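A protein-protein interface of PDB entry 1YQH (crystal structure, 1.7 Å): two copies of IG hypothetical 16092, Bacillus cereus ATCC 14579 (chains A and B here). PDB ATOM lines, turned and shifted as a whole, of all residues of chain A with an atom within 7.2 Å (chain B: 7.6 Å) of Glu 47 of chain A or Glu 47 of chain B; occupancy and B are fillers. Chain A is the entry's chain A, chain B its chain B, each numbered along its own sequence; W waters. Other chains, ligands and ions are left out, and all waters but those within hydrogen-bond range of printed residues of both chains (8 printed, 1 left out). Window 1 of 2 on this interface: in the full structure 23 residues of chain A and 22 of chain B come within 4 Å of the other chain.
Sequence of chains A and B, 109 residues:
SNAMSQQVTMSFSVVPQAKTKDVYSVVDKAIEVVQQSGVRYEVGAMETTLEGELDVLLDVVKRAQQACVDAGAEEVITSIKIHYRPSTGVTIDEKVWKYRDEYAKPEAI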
ATOM      1  N   MET A  10     -23.332  22.598  -8.138  1.00  0.00           N
ATOM      2  CA  MET A  10     -22.131  22.260  -7.389  1.00  0.00           C
ATOM      3  C   MET A  10     -21.671  20.878  -7.849  1.00  0.00           C
ATOM      4  O   MET A  10     -22.489  20.075  -8.306  1.00  0.00           O
ATOM      5  CB  MET A  10     -22.501  22.219  -5.904  1.00  0.00           C
ATOM      6  CG  MET A  10     -21.367  21.997  -4.941  1.00  0.00           C
ATOM      7  SD  MET A  10     -22.090  21.874  -3.147  1.00  0.00           S
ATOM      8  CE  MET A  10     -22.790  23.707  -2.933  1.00  0.00           C
ATOM      9  N   SER A  11     -20.368  20.615  -7.781  1.00  0.00           N
ATOM     10  CA  SER A  11     -19.903  19.245  -7.825  1.00  0.00           C
ATOM     11  C   SER A  11     -19.033  18.968  -6.624  1.00  0.00           C
ATOM     12  O   SER A  11     -18.477  19.897  -6.017  1.00  0.00           O
ATOM     13  CB  SER A  11     -19.157  18.931  -9.131  1.00  0.00           C
ATOM     14  OG  SER A  11     -17.939  19.645  -9.214  1.00  0.00           O
ATOM     15  N   PHE A  12     -18.930  17.698  -6.256  1.00  0.00           N
ATOM     16  CA  PHE A  12     -18.053  17.340  -5.155  1.00  0.00           C
ATOM     17  C   PHE A  12     -17.569  15.921  -5.303  1.00  0.00           C
ATOM     18  O   PHE A  12     -18.173  15.096  -6.013  1.00  0.00           O
ATOM     19  CB  PHE A  12     -18.776  17.526  -3.795  1.00  0.00           C
ATOM     20  CG  PHE A  12     -19.604  16.332  -3.365  1.00  0.00           C
ATOM     21  CD1 PHE A  12     -19.121  15.444  -2.395  1.00  0.00           C
ATOM     22  CD2 PHE A  12     -20.866  16.095  -3.922  1.00  0.00           C
ATOM     23  CE1 PHE A  12     -19.869  14.342  -1.984  1.00  0.00           C
ATOM     24  CE2 PHE A  12     -21.625  14.996  -3.513  1.00  0.00           C
ATOM     25  CZ  PHE A  12     -21.131  14.115  -2.546  1.00  0.00           C
ATOM     26  N   SER A  13     -16.476  15.636  -4.616  1.00  0.00           N
ATOM     27  CA  SER A  13     -15.996  14.271  -4.505  1.00  0.00           C
ATOM     28  C   SER A  13     -15.400  14.047  -3.126  1.00  0.00           C
ATOM     29  O   SER A  13     -14.978  15.006  -2.472  1.00  0.00           O
ATOM     30  CB  SER A  13     -14.969  13.982  -5.603  1.00  0.00           C
ATOM     31  OG  SER A  13     -13.908  14.913  -5.555  1.00  0.00           O
ATOM     32  N   VAL A  14     -15.383  12.782  -2.698  1.00  0.00           N
ATOM     33  CA  VAL A  14     -14.714  12.374  -1.457  1.00  0.00           C
ATOM     34  C   VAL A  14     -13.684  11.304  -1.780  1.00  0.00           C
ATOM     35  O   VAL A  14     -13.968  10.356  -2.527  1.00  0.00           O
ATOM     36  CB  VAL A  14     -15.736  11.872  -0.396  1.00  0.00           C
ATOM     37  CG1 VAL A  14     -16.575  13.041   0.116  1.00  0.00           C
ATOM     38  CG2 VAL A  14     -16.643  10.788  -0.991  1.00  0.00           C
ATOM     39  N   ILE A  31     -22.295   8.434  -1.476  1.00  0.00           N
ATOM     40  CA  ILE A  31     -23.285   8.614  -2.551  1.00  0.00           C
ATOM     41  C   ILE A  31     -24.708   8.338  -2.037  1.00  0.00           C
ATOM     42  O   ILE A  31     -25.666   8.995  -2.461  1.00  0.00           O
ATOM     43  CB  ILE A  31     -22.920   7.776  -3.801  1.00  0.00           C
ATOM     44  CG1 ILE A  31     -21.550   8.205  -4.355  1.00  0.00           C
ATOM     45  CG2 ILE A  31     -24.018   7.888  -4.874  1.00  0.00           C
ATOM     46  CD1 ILE A  31     -21.472   9.649  -4.780  1.00  0.00           C
ATOM     47  N   GLU A  42     -26.285  14.092 -10.397  1.00  0.00           N
ATOM     48  CA  GLU A  42     -25.749  13.127 -11.337  1.00  0.00           C
ATOM     49  C   GLU A  42     -24.360  12.716 -10.892  1.00  0.00           C
ATOM     50  O   GLU A  42     -23.494  13.567 -10.694  1.00  0.00           O
ATOM     51  CB  GLU A  42     -25.690  13.713 -12.738  1.00  0.00           C
ATOM     52  CG  GLU A  42     -25.265  12.708 -13.794  1.00  0.00           C
ATOM     53  CD  GLU A  42     -25.159  13.355 -15.155  1.00  0.00           C
ATOM     54  OE1 GLU A  42     -25.999  13.040 -16.017  1.00  0.00           O
ATOM     55  OE2 GLU A  42     -24.267  14.207 -15.347  1.00  0.00           O
ATOM     56  N   VAL A  43     -24.174  11.413 -10.726  1.00  0.00           N
ATOM     57  CA  VAL A  43     -22.876  10.860 -10.377  1.00  0.00           C
ATOM     58  C   VAL A  43     -22.010  10.750 -11.643  1.00  0.00           C
ATOM     59  O   VAL A  43     -22.413  10.139 -12.644  1.00  0.00           O
ATOM     60  CB  VAL A  43     -23.021   9.486  -9.673  1.00  0.00           C
ATOM     61  CG1 VAL A  43     -21.639   8.920  -9.333  1.00  0.00           C
ATOM     62  CG2 VAL A  43     -23.866   9.623  -8.385  1.00  0.00           C
ATOM     63  N   GLY A  44     -20.848  11.398 -11.601  1.00  0.00           N
ATOM     64  CA  GLY A  44     -19.854  11.274 -12.680  1.00  0.00           C
ATOM     65  C   GLY A  44     -18.669  10.459 -12.206  1.00  0.00           C
ATOM     66  O   GLY A  44     -18.568  10.096 -11.023  1.00  0.00           O
ATOM     67  N   ALA A  45     -17.758  10.164 -13.133  1.00  0.00           N
ATOM     68  CA  ALA A  45     -16.611   9.307 -12.818  1.00  0.00           C
ATOM     69  C   ALA A  45     -15.662   9.943 -11.793  1.00  0.00           C
ATOM     70  O   ALA A  45     -15.021   9.218 -11.029  1.00  0.00           O
ATOM     71  CB  ALA A  45     -15.850   8.978 -14.093  1.00  0.00           C
ATOM     72  N   MET A  46     -15.586  11.276 -11.779  1.00  0.00           N
ATOM     73  CA  MET A  46     -14.636  12.005 -10.904  1.00  0.00           C
ATOM     74  C   MET A  46     -15.299  12.882  -9.841  1.00  0.00           C
ATOM     75  O   MET A  46     -14.680  13.182  -8.815  1.00  0.00           O
ATOM     76  CB  MET A  46     -13.691  12.902 -11.741  1.00  0.00           C
ATOM     77  CG  MET A  46     -12.883  12.142 -12.829  1.00  0.00           C
ATOM     78  SD  MET A  46     -11.723  10.776 -12.094  1.00  0.00           S
ATOM     79  CE  MET A  46     -10.484  11.952 -11.193  1.00  0.00           C
ATOM     80  N   GLU A  47     -16.546  13.289 -10.110  1.00  0.00           N
ATOM     81  CA  GLU A  47     -17.302  14.253  -9.294  1.00  0.00           C
ATOM     82  C   GLU A  47     -18.793  13.935  -9.392  1.00  0.00           C
ATOM     83  O   GLU A  47     -19.249  13.436 -10.424  1.00  0.00           O
ATOM     84  CB  GLU A  47     -17.108  15.697  -9.815  1.00  0.00           C
ATOM     85  CG  GLU A  47     -15.673  16.193 -10.037  1.00  0.00           C
ATOM     86  CD  GLU A  47     -14.804  16.180  -8.780  1.00  0.00           C
ATOM     87  OE1 GLU A  47     -15.321  16.281  -7.643  1.00  0.00           O
ATOM     88  OE2 GLU A  47     -13.576  16.067  -8.940  1.00  0.00           O
ATOM     89  N   THR A  48     -19.547  14.235  -8.331  1.00  0.00           N
ATOM     90  CA  THR A  48     -21.012  14.142  -8.364  1.00  0.00           C
ATOM     91  C   THR A  48     -21.543  15.560  -8.432  1.00  0.00           C
ATOM     92  O   THR A  48     -21.113  16.423  -7.644  1.00  0.00           O
ATOM     93  CB  THR A  48     -21.525  13.414  -7.102  1.00  0.00           C
ATOM     94  OG1 THR A  48     -21.163  12.036  -7.209  1.00  0.00           O
ATOM     95  CG2 THR A  48     -23.064  13.528  -6.934  1.00  0.00           C
ATOM     96  N   THR A  49     -22.449  15.801  -9.378  1.00  0.00           N
ATOM     97  CA  THR A  49     -23.050  17.120  -9.572  1.00  0.00           C
ATOM     98  C   THR A  49     -24.349  17.190  -8.774  1.00  0.00           C
ATOM     99  O   THR A  49     -25.107  16.218  -8.776  1.00  0.00           O
ATOM    100  CB  THR A  49     -23.369  17.357 -11.062  1.00  0.00           C
ATOM    101  OG1 THR A  49     -22.175  17.168 -11.830  1.00  0.00           O
ATOM    102  CG2 THR A  49     -23.898  18.791 -11.276  1.00  0.00           C
ATOM    103  N   SER A  79     -13.479  17.502  -2.137  1.00  0.00           N
ATOM    104  CA  SER A  79     -13.331  18.588  -3.106  1.00  0.00           C
ATOM    105  C   SER A  79     -14.726  19.088  -3.466  1.00  0.00           C
ATOM    106  O   SER A  79     -15.658  18.296  -3.600  1.00  0.00           O
ATOM    107  CB  SER A  79     -12.630  18.103  -4.377  1.00  0.00           C
ATOM    108  OG  SER A  79     -11.355  17.537  -4.101  1.00  0.00           O
ATOM    109  N   ILE A  80     -14.862  20.395  -3.620  1.00  0.00           N
ATOM    110  CA  ILE A  80     -16.144  21.007  -3.940  1.00  0.00           C
ATOM    111  C   ILE A  80     -15.892  22.088  -4.978  1.00  0.00           C
ATOM    112  O   ILE A  80     -14.886  22.804  -4.900  1.00  0.00           O
ATOM    113  CB  ILE A  80     -16.814  21.669  -2.684  1.00  0.00           C
ATOM    114  CG1 ILE A  80     -16.969  20.661  -1.537  1.00  0.00           C
ATOM    115  CG2 ILE A  80     -18.176  22.274  -3.058  1.00  0.00           C
ATOM    116  CD1 ILE A  80     -17.305  21.270  -0.173  1.00  0.00           C
ATOM    117  N   LYS A  81     -16.786  22.185  -5.965  1.00  0.00           N
ATOM    118  CA  LYS A  81     -16.786  23.334  -6.856  1.00  0.00           C
ATOM    119  C   LYS A  81     -18.208  23.889  -6.901  1.00  0.00           C
ATOM    120  O   LYS A  81     -19.167  23.127  -7.082  1.00  0.00           O
ATOM    121  CB  LYS A  81     -16.335  22.938  -8.255  1.00  0.00           C
ATOM    122  CG  LYS A  81     -15.816  24.114  -9.075  1.00  0.00           C
ATOM    123  CD  LYS A  81     -15.137  23.645 -10.357  1.00  0.00           C
ATOM    124  CE  LYS A  81     -13.683  23.185 -10.144  1.00  0.00           C
ATOM    125  NZ  LYS A  81     -12.712  24.306  -9.909  1.00  0.00           N
ATOM    126  N   LYS A  95     -26.045  24.641 -18.421  1.00  0.00           N
ATOM    127  CA  LYS A  95     -24.631  24.407 -18.701  1.00  0.00           C
ATOM    128  C   LYS A  95     -24.359  23.238 -19.646  1.00  0.00           C
ATOM    129  O   LYS A  95     -23.360  23.259 -20.365  1.00  0.00           O
ATOM    130  CB  LYS A  95     -23.845  24.278 -17.394  1.00  0.00           C
ATOM    131  CG  LYS A  95     -24.032  25.533 -16.520  1.00  0.00           C
ATOM    132  CD  LYS A  95     -23.060  25.622 -15.376  1.00  0.00           C
ATOM    133  CE  LYS A  95     -21.699  26.081 -15.837  1.00  0.00           C
ATOM    134  NZ  LYS A  95     -20.706  25.828 -14.749  1.00  0.00           N
ATOM    135  N   VAL A  96     -25.252  22.250 -19.688  1.00  0.00           N
ATOM    136  CA  VAL A  96     -24.975  21.028 -20.463  1.00  0.00           C
ATOM    137  C   VAL A  96     -25.838  20.807 -21.710  1.00  0.00           C
ATOM    138  O   VAL A  96     -25.543  19.918 -22.495  1.00  0.00           O
ATOM    139  CB  VAL A  96     -25.050  19.737 -19.587  1.00  0.00           C
ATOM    140  CG1 VAL A  96     -24.142  19.851 -18.380  1.00  0.00           C
ATOM    141  CG2 VAL A  96     -26.491  19.431 -19.171  1.00  0.00           C
ATOM    142  N   ARG A 100     -25.116  17.607 -24.872  1.00  0.00           N
ATOM    143  CA  ARG A 100     -25.636  16.273 -24.661  1.00  0.00           C
ATOM    144  C   ARG A 100     -26.769  15.954 -25.626  1.00  0.00           C
ATOM    145  O   ARG A 100     -27.708  16.737 -25.774  1.00  0.00           O
ATOM    146  CB  ARG A 100     -26.127  16.123 -23.226  1.00  0.00           C
ATOM    147  CG  ARG A 100     -25.019  16.217 -22.205  1.00  0.00           C
ATOM    148  CD  ARG A 100     -25.502  15.667 -20.916  1.00  0.00           C
ATOM    149  NE  ARG A 100     -24.450  15.629 -19.910  1.00  0.00           N
ATOM    150  CZ  ARG A 100     -24.557  14.962 -18.769  1.00  0.00           C
ATOM    151  NH1 ARG A 100     -25.665  14.267 -18.512  1.00  0.00           N
ATOM    152  NH2 ARG A 100     -23.566  14.977 -17.895  1.00  0.00           N
ATOM    153  N   MET B  10     -10.236  11.334 -16.469  1.00  0.00           N
ATOM    154  CA  MET B  10      -9.801  12.679 -16.130  1.00  0.00           C
ATOM    155  C   MET B  10     -11.017  13.582 -16.208  1.00  0.00           C
ATOM    156  O   MET B  10     -11.891  13.372 -17.047  1.00  0.00           O
ATOM    157  CB  MET B  10      -8.752  13.131 -17.145  1.00  0.00           C
ATOM    158  CG  MET B  10      -8.143  14.493 -16.879  1.00  0.00           C
ATOM    159  SD  MET B  10      -6.796  14.915 -18.227  1.00  0.00           S
ATOM    160  CE  MET B  10      -5.515  13.381 -17.887  1.00  0.00           C
ATOM    161  N   SER B  11     -11.094  14.576 -15.340  1.00  0.00           N
ATOM    162  CA  SER B  11     -12.062  15.636 -15.561  1.00  0.00           C
ATOM    163  C   SER B  11     -11.327  16.955 -15.625  1.00  0.00           C
ATOM    164  O   SER B  11     -10.215  17.086 -15.089  1.00  0.00           O
ATOM    165  CB  SER B  11     -13.140  15.644 -14.470  1.00  0.00           C
ATOM    166  OG  SER B  11     -12.540  15.816 -13.198  1.00  0.00           O
ATOM    167  N   PHE B  12     -11.927  17.939 -16.286  1.00  0.00           N
ATOM    168  CA  PHE B  12     -11.308  19.242 -16.327  1.00  0.00           C
ATOM    169  C   PHE B  12     -12.349  20.311 -16.530  1.00  0.00           C
ATOM    170  O   PHE B  12     -13.452  20.047 -17.000  1.00  0.00           O
ATOM    171  CB  PHE B  12     -10.233  19.326 -17.440  1.00  0.00           C
ATOM    172  CG  PHE B  12     -10.782  19.640 -18.818  1.00  0.00           C
ATOM    173  CD1 PHE B  12     -10.665  20.923 -19.356  1.00  0.00           C
ATOM    174  CD2 PHE B  12     -11.421  18.661 -19.566  1.00  0.00           C
ATOM    175  CE1 PHE B  12     -11.170  21.219 -20.623  1.00  0.00           C
ATOM    176  CE2 PHE B  12     -11.921  18.939 -20.832  1.00  0.00           C
ATOM    177  CZ  PHE B  12     -11.814  20.209 -21.359  1.00  0.00           C
ATOM    178  N   SER B  13     -11.961  21.530 -16.201  1.00  0.00           N
ATOM    179  CA  SER B  13     -12.775  22.675 -16.499  1.00  0.00           C
ATOM    180  C   SER B  13     -11.880  23.853 -16.845  1.00  0.00           C
ATOM    181  O   SER B  13     -10.702  23.905 -16.455  1.00  0.00           O
ATOM    182  CB  SER B  13     -13.696  22.999 -15.322  1.00  0.00           C
ATOM    183  OG  SER B  13     -12.949  23.316 -14.171  1.00  0.00           O
ATOM    184  N   VAL B  14     -12.451  24.775 -17.610  1.00  0.00           N
ATOM    185  CA  VAL B  14     -11.782  26.025 -17.935  1.00  0.00           C
ATOM    186  C   VAL B  14     -12.691  27.172 -17.532  1.00  0.00           C
ATOM    187  O   VAL B  14     -13.896  27.177 -17.838  1.00  0.00           O
ATOM    188  CB  VAL B  14     -11.403  26.100 -19.438  1.00  0.00           C
ATOM    189  CG1 VAL B  14     -10.242  25.150 -19.740  1.00  0.00           C
ATOM    190  CG2 VAL B  14     -12.611  25.745 -20.327  1.00  0.00           C
ATOM    191  N   GLU B  42     -17.794  13.062 -21.506  1.00  0.00           N
ATOM    192  CA  GLU B  42     -19.118  13.536 -21.131  1.00  0.00           C
ATOM    193  C   GLU B  42     -19.000  14.920 -20.526  1.00  0.00           C
ATOM    194  O   GLU B  42     -18.207  15.122 -19.598  1.00  0.00           O
ATOM    195  CB  GLU B  42     -19.782  12.585 -20.127  1.00  0.00           C
ATOM    196  CG  GLU B  42     -21.237  12.957 -19.868  1.00  0.00           C
ATOM    197  CD  GLU B  42     -21.897  12.065 -18.844  1.00  0.00           C
ATOM    198  OE1 GLU B  42     -22.963  11.500 -19.172  1.00  0.00           O
ATOM    199  OE2 GLU B  42     -21.359  11.939 -17.722  1.00  0.00           O
ATOM    200  N   VAL B  43     -19.769  15.867 -21.060  1.00  0.00           N
ATOM    201  CA  VAL B  43     -19.783  17.210 -20.518  1.00  0.00           C
ATOM    202  C   VAL B  43     -20.718  17.223 -19.306  1.00  0.00           C
ATOM    203  O   VAL B  43     -21.888  16.824 -19.411  1.00  0.00           O
ATOM    204  CB  VAL B  43     -20.221  18.257 -21.566  1.00  0.00           C
ATOM    205  CG1 VAL B  43     -20.297  19.655 -20.927  1.00  0.00           C
ATOM    206  CG2 VAL B  43     -19.238  18.263 -22.749  1.00  0.00           C
ATOM    207  N   GLY B  44     -20.178  17.654 -18.169  1.00  0.00           N
ATOM    208  CA  GLY B  44     -20.973  17.873 -16.946  1.00  0.00           C
ATOM    209  C   GLY B  44     -21.142  19.362 -16.697  1.00  0.00           C
ATOM    210  O   GLY B  44     -20.509  20.192 -17.360  1.00  0.00           O
ATOM    211  N   ALA B  45     -22.013  19.709 -15.750  1.00  0.00           N
ATOM    212  CA  ALA B  45     -22.268  21.112 -15.438  1.00  0.00           C
ATOM    213  C   ALA B  45     -21.031  21.862 -14.934  1.00  0.00           C
ATOM    214  O   ALA B  45     -20.884  23.051 -15.222  1.00  0.00           O
ATOM    215  CB  ALA B  45     -23.418  21.245 -14.417  1.00  0.00           C
ATOM    216  N   MET B  46     -20.169  21.187 -14.168  1.00  0.00           N
ATOM    217  CA  MET B  46     -19.010  21.844 -13.553  1.00  0.00           C
ATOM    218  C   MET B  46     -17.673  21.424 -14.148  1.00  0.00           C
ATOM    219  O   MET B  46     -16.673  22.141 -14.012  1.00  0.00           O
ATOM    220  CB  MET B  46     -18.947  21.587 -12.034  1.00  0.00           C
ATOM    221  CG  MET B  46     -20.173  22.009 -11.236  1.00  0.00           C
ATOM    222  SD  MET B  46     -20.604  23.895 -11.468  1.00  0.00           S
ATOM    223  CE  MET B  46     -18.954  24.725 -10.743  1.00  0.00           C
ATOM    224  N   GLU B  47     -17.653  20.266 -14.793  1.00  0.00           N
ATOM    225  CA  GLU B  47     -16.433  19.762 -15.419  1.00  0.00           C
ATOM    226  C   GLU B  47     -16.765  18.729 -16.483  1.00  0.00           C
ATOM    227  O   GLU B  47     -17.842  18.126 -16.464  1.00  0.00           O
ATOM    228  CB  GLU B  47     -15.461  19.178 -14.373  1.00  0.00           C
ATOM    229  CG  GLU B  47     -15.988  17.996 -13.545  1.00  0.00           C
ATOM    230  CD  GLU B  47     -16.919  18.421 -12.400  1.00  0.00           C
ATOM    231  OE1 GLU B  47     -16.559  19.338 -11.633  1.00  0.00           O
ATOM    232  OE2 GLU B  47     -18.004  17.826 -12.259  1.00  0.00           O
ATOM    233  N   THR B  48     -15.829  18.534 -17.404  1.00  0.00           N
ATOM    234  CA  THR B  48     -15.998  17.581 -18.497  1.00  0.00           C
ATOM    235  C   THR B  48     -15.098  16.378 -18.214  1.00  0.00           C
ATOM    236  O   THR B  48     -13.911  16.548 -17.869  1.00  0.00           O
ATOM    237  CB  THR B  48     -15.647  18.250 -19.832  1.00  0.00           C
ATOM    238  OG1 THR B  48     -16.679  19.185 -20.150  1.00  0.00           O
ATOM    239  CG2 THR B  48     -15.522  17.252 -20.982  1.00  0.00           C
ATOM    240  N   THR B  49     -15.667  15.182 -18.367  1.00  0.00           N
ATOM    241  CA  THR B  49     -14.968  13.933 -18.065  1.00  0.00           C
ATOM    242  C   THR B  49     -14.438  13.328 -19.360  1.00  0.00           C
ATOM    243  O   THR B  49     -15.156  13.315 -20.359  1.00  0.00           O
ATOM    244  CB  THR B  49     -15.893  12.930 -17.355  1.00  0.00           C
ATOM    245  OG1 THR B  49     -16.353  13.519 -16.130  1.00  0.00           O
ATOM    246  CG2 THR B  49     -15.134  11.645 -17.009  1.00  0.00           C
ATOM    247  N   LEU B  50     -13.192  12.849 -19.311  1.00  0.00           N
ATOM    248  CA  LEU B  50     -12.498  12.209 -20.428  1.00  0.00           C
ATOM    249  C   LEU B  50     -12.021  10.814 -20.030  1.00  0.00           C
ATOM    250  O   LEU B  50     -11.682  10.568 -18.877  1.00  0.00           O
ATOM    251  CB  LEU B  50     -11.262  13.016 -20.824  1.00  0.00           C
ATOM    252  CG  LEU B  50     -11.411  14.529 -21.068  1.00  0.00           C
ATOM    253  CD1 LEU B  50     -10.061  15.198 -21.319  1.00  0.00           C
ATOM    254  CD2 LEU B  50     -12.411  14.846 -22.189  1.00  0.00           C
ATOM    255  N   SER B  79      -8.700  23.689 -14.404  1.00  0.00           N
ATOM    256  CA  SER B  79      -8.667  22.695 -13.321  1.00  0.00           C
ATOM    257  C   SER B  79      -8.677  21.296 -13.930  1.00  0.00           C
ATOM    258  O   SER B  79      -9.382  21.045 -14.902  1.00  0.00           O
ATOM    259  CB  SER B  79      -9.865  22.863 -12.382  1.00  0.00           C
ATOM    260  OG  SER B  79      -9.883  24.152 -11.798  1.00  0.00           O
ATOM    261  N   ILE B  80      -7.897  20.386 -13.357  1.00  0.00           N
ATOM    262  CA  ILE B  80      -7.775  19.033 -13.897  1.00  0.00           C
ATOM    263  C   ILE B  80      -7.782  18.070 -12.723  1.00  0.00           C
ATOM    264  O   ILE B  80      -7.221  18.374 -11.669  1.00  0.00           O
ATOM    265  CB  ILE B  80      -6.434  18.814 -14.673  1.00  0.00           C
ATOM    266  CG1 ILE B  80      -6.224  19.874 -15.760  1.00  0.00           C
ATOM    267  CG2 ILE B  80      -6.411  17.428 -15.306  1.00  0.00           C
ATOM    268  CD1 ILE B  80      -4.830  19.893 -16.348  1.00  0.00           C
ATOM    269  N   LYS B  81      -8.413  16.914 -12.913  1.00  0.00           N
ATOM    270  CA  LYS B  81      -8.277  15.825 -11.952  1.00  0.00           C
ATOM    271  C   LYS B  81      -8.106  14.508 -12.686  1.00  0.00           C
ATOM    272  O   LYS B  81      -8.838  14.237 -13.649  1.00  0.00           O
ATOM    273  CB  LYS B  81      -9.483  15.768 -11.036  1.00  0.00           C
ATOM    274  CG  LYS B  81      -9.264  14.853  -9.835  1.00  0.00           C
ATOM    275  CD  LYS B  81     -10.442  14.956  -8.885  1.00  0.00           C
ATOM    276  CE  LYS B  81     -10.445  16.315  -8.183  1.00  0.00           C
ATOM    277  NZ  LYS B  81     -11.491  16.391  -7.121  1.00  0.00           N
ATOM    278  N   LYS B  95     -16.518   3.406 -12.531  1.00  0.00           N
ATOM    279  CA  LYS B  95     -16.799   4.347 -11.449  1.00  0.00           C
ATOM    280  C   LYS B  95     -18.281   4.693 -11.318  1.00  0.00           C
ATOM    281  O   LYS B  95     -18.747   4.979 -10.210  1.00  0.00           O
ATOM    282  CB  LYS B  95     -15.937   5.598 -11.603  1.00  0.00           C
ATOM    283  CG  LYS B  95     -14.446   5.247 -11.741  1.00  0.00           C
ATOM    284  CD  LYS B  95     -13.520   6.368 -11.356  1.00  0.00           C
ATOM    285  CE  LYS B  95     -13.547   6.684  -9.866  1.00  0.00           C
ATOM    286  NZ  LYS B  95     -12.860   8.001  -9.682  1.00  0.00           N
ATOM    287  N   VAL B  96     -19.032   4.629 -12.421  1.00  0.00           N
ATOM    288  CA  VAL B  96     -20.425   5.091 -12.402  1.00  0.00           C
ATOM    289  C   VAL B  96     -21.527   4.030 -12.503  1.00  0.00           C
ATOM    290  O   VAL B  96     -22.687   4.357 -12.287  1.00  0.00           O
ATOM    291  CB  VAL B  96     -20.708   6.185 -13.478  1.00  0.00           C
ATOM    292  CG1 VAL B  96     -19.717   7.340 -13.353  1.00  0.00           C
ATOM    293  CG2 VAL B  96     -20.691   5.588 -14.864  1.00  0.00           C
ATOM    294  N   ARG B 100     -26.006   5.037 -11.916  1.00  0.00           N
ATOM    295  CA  ARG B 100     -26.830   5.562 -12.991  1.00  0.00           C
ATOM    296  C   ARG B 100     -27.802   4.505 -13.500  1.00  0.00           C
ATOM    297  O   ARG B 100     -27.404   3.364 -13.729  1.00  0.00           O
ATOM    298  CB  ARG B 100     -25.943   6.026 -14.135  1.00  0.00           C
ATOM    299  CG  ARG B 100     -25.149   7.275 -13.821  1.00  0.00           C
ATOM    300  CD  ARG B 100     -24.504   7.769 -15.091  1.00  0.00           C
ATOM    301  NE  ARG B 100     -23.706   8.964 -14.874  1.00  0.00           N
ATOM    302  CZ  ARG B 100     -23.356   9.812 -15.839  1.00  0.00           C
ATOM    303  NH1 ARG B 100     -22.622  10.874 -15.542  1.00  0.00           N
ATOM    304  NH2 ARG B 100     -23.742   9.599 -17.098  1.00  0.00           N
HETATM  305  O   HOH W   1     -23.370  17.519 -14.605  1.00  0.00           O
HETATM  306  O   HOH W   2     -20.362  18.685 -13.196  1.00  0.00           O
HETATM  307  O   HOH W   3     -21.825  13.559 -14.351  1.00  0.00           O
HETATM  308  O   HOH W   4     -18.446  10.935 -15.740  1.00  0.00           O
HETATM  309  O   HOH W   5     -11.214  14.142  -5.729  1.00  0.00           O
HETATM  310  O   HOH W   6     -20.855  14.522 -16.662  1.00  0.00           O
HETATM  311  O   HOH W   7     -12.813  17.508 -11.206  1.00  0.00           O
HETATM  312  O   HOH W   8     -13.625  25.375 -12.569  1.00  0.00           O
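The backbone carbonyl oxygen of Glu 42 of chain A is in hydrogen-bond range of the backbone NH of Thr 49 of chain A, at 2.8 Å.
Hydrophobic or aromatic side chains of chain B within 4 Å of the printed part of chain A: Met 46 and Val 96.
C of Met 10 of chain A touches CG of Met 46 of chain B, 3.9 Å away. O of Val 43 of chain A touches CG1 of Val 96 of chain B (3.95 Å). Lys 81 of chain A touches Met 46 of chain B (CG to CE, 3.6 Å). Val 96 of chain A touches Val 43 of chain B.
OG of Ser 11 of chain A is in hydrogen-bond range of OE1 of Glu 47 of chain B. The side-chain hydroxyl (OG) of Ser 13 of chain A lies within hydrogen-bond range of the side-chain amino group (NZ) of Lys 81 of chain B, 3.2 Å away. The guanidinium group (NH1) of Arg 100 of chain B lies within salt-bridge range of the side-chain carboxylate (OE2) of Glu 42 of chain A (3.7 Å). The backbone carbonyl oxygen (O) of Ala 45 of chain A is in hydrogen-bond range of the side-chain amino group (NZ) of Lys 95 of chain B (2.8 Å). NZ of Lys 81 of chain B lies within salt-bridge range of OE2 of Glu 47 of chain A. The side-chain hydroxyl (OG) of Ser 79 of chain A is in hydrogen-bond range of the side-chain amino group (NZ) of Lys 81 of chain B (3.2 Å). The side-chain amino group of Lys 81 of chain A sits at hydrogen-bond distance from the side-chain hydroxyl of Ser 79 of chain B, 3.4 Å away. The side-chain amino group (NZ) of Lys 95 of chain A sits at hydrogen-bond distance from the backbone carbonyl oxygen (O) of Ala 45 of chain B (2.8 Å). The guanidinium group of Arg 100 of chain A is in salt-bridge range of the side-chain carboxylate of Glu 42 of chain B (3.8 Å). NE of Arg 100 of chain A lies within hydrogen-bond range of O of Val 43 of chain B (2.9 Å).
Water W8 lies within hydrogen-bond range of OG of Ser 13 of chain B and NZ of Lys 81 of chain A. Water W1 lies within hydrogen-bond range of the backbone NH (N) of Ala 45 of chain B and the side-chain hydroxyl (OG1) of Thr 49 of chain A.
Ala 45 of chain A touches Lys 95 of chain B, and with the chains exchanged Lys 95 of chain A touches Ala 45 of chain B. 19 positions are printed for both chains.
Printed residues of chain A within 4 Å of Glu 47 of chain B: Ser 11 and Glu 47. Of the printed residues of chain B, Lys 95 of chain A touches Ala 45 (2.8 Å) and Met 46 (3.8 Å). The nearest printed residue of chain B that does not touch Glu 47 of chain A is Ser 11 of chain B (4.4 Å).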
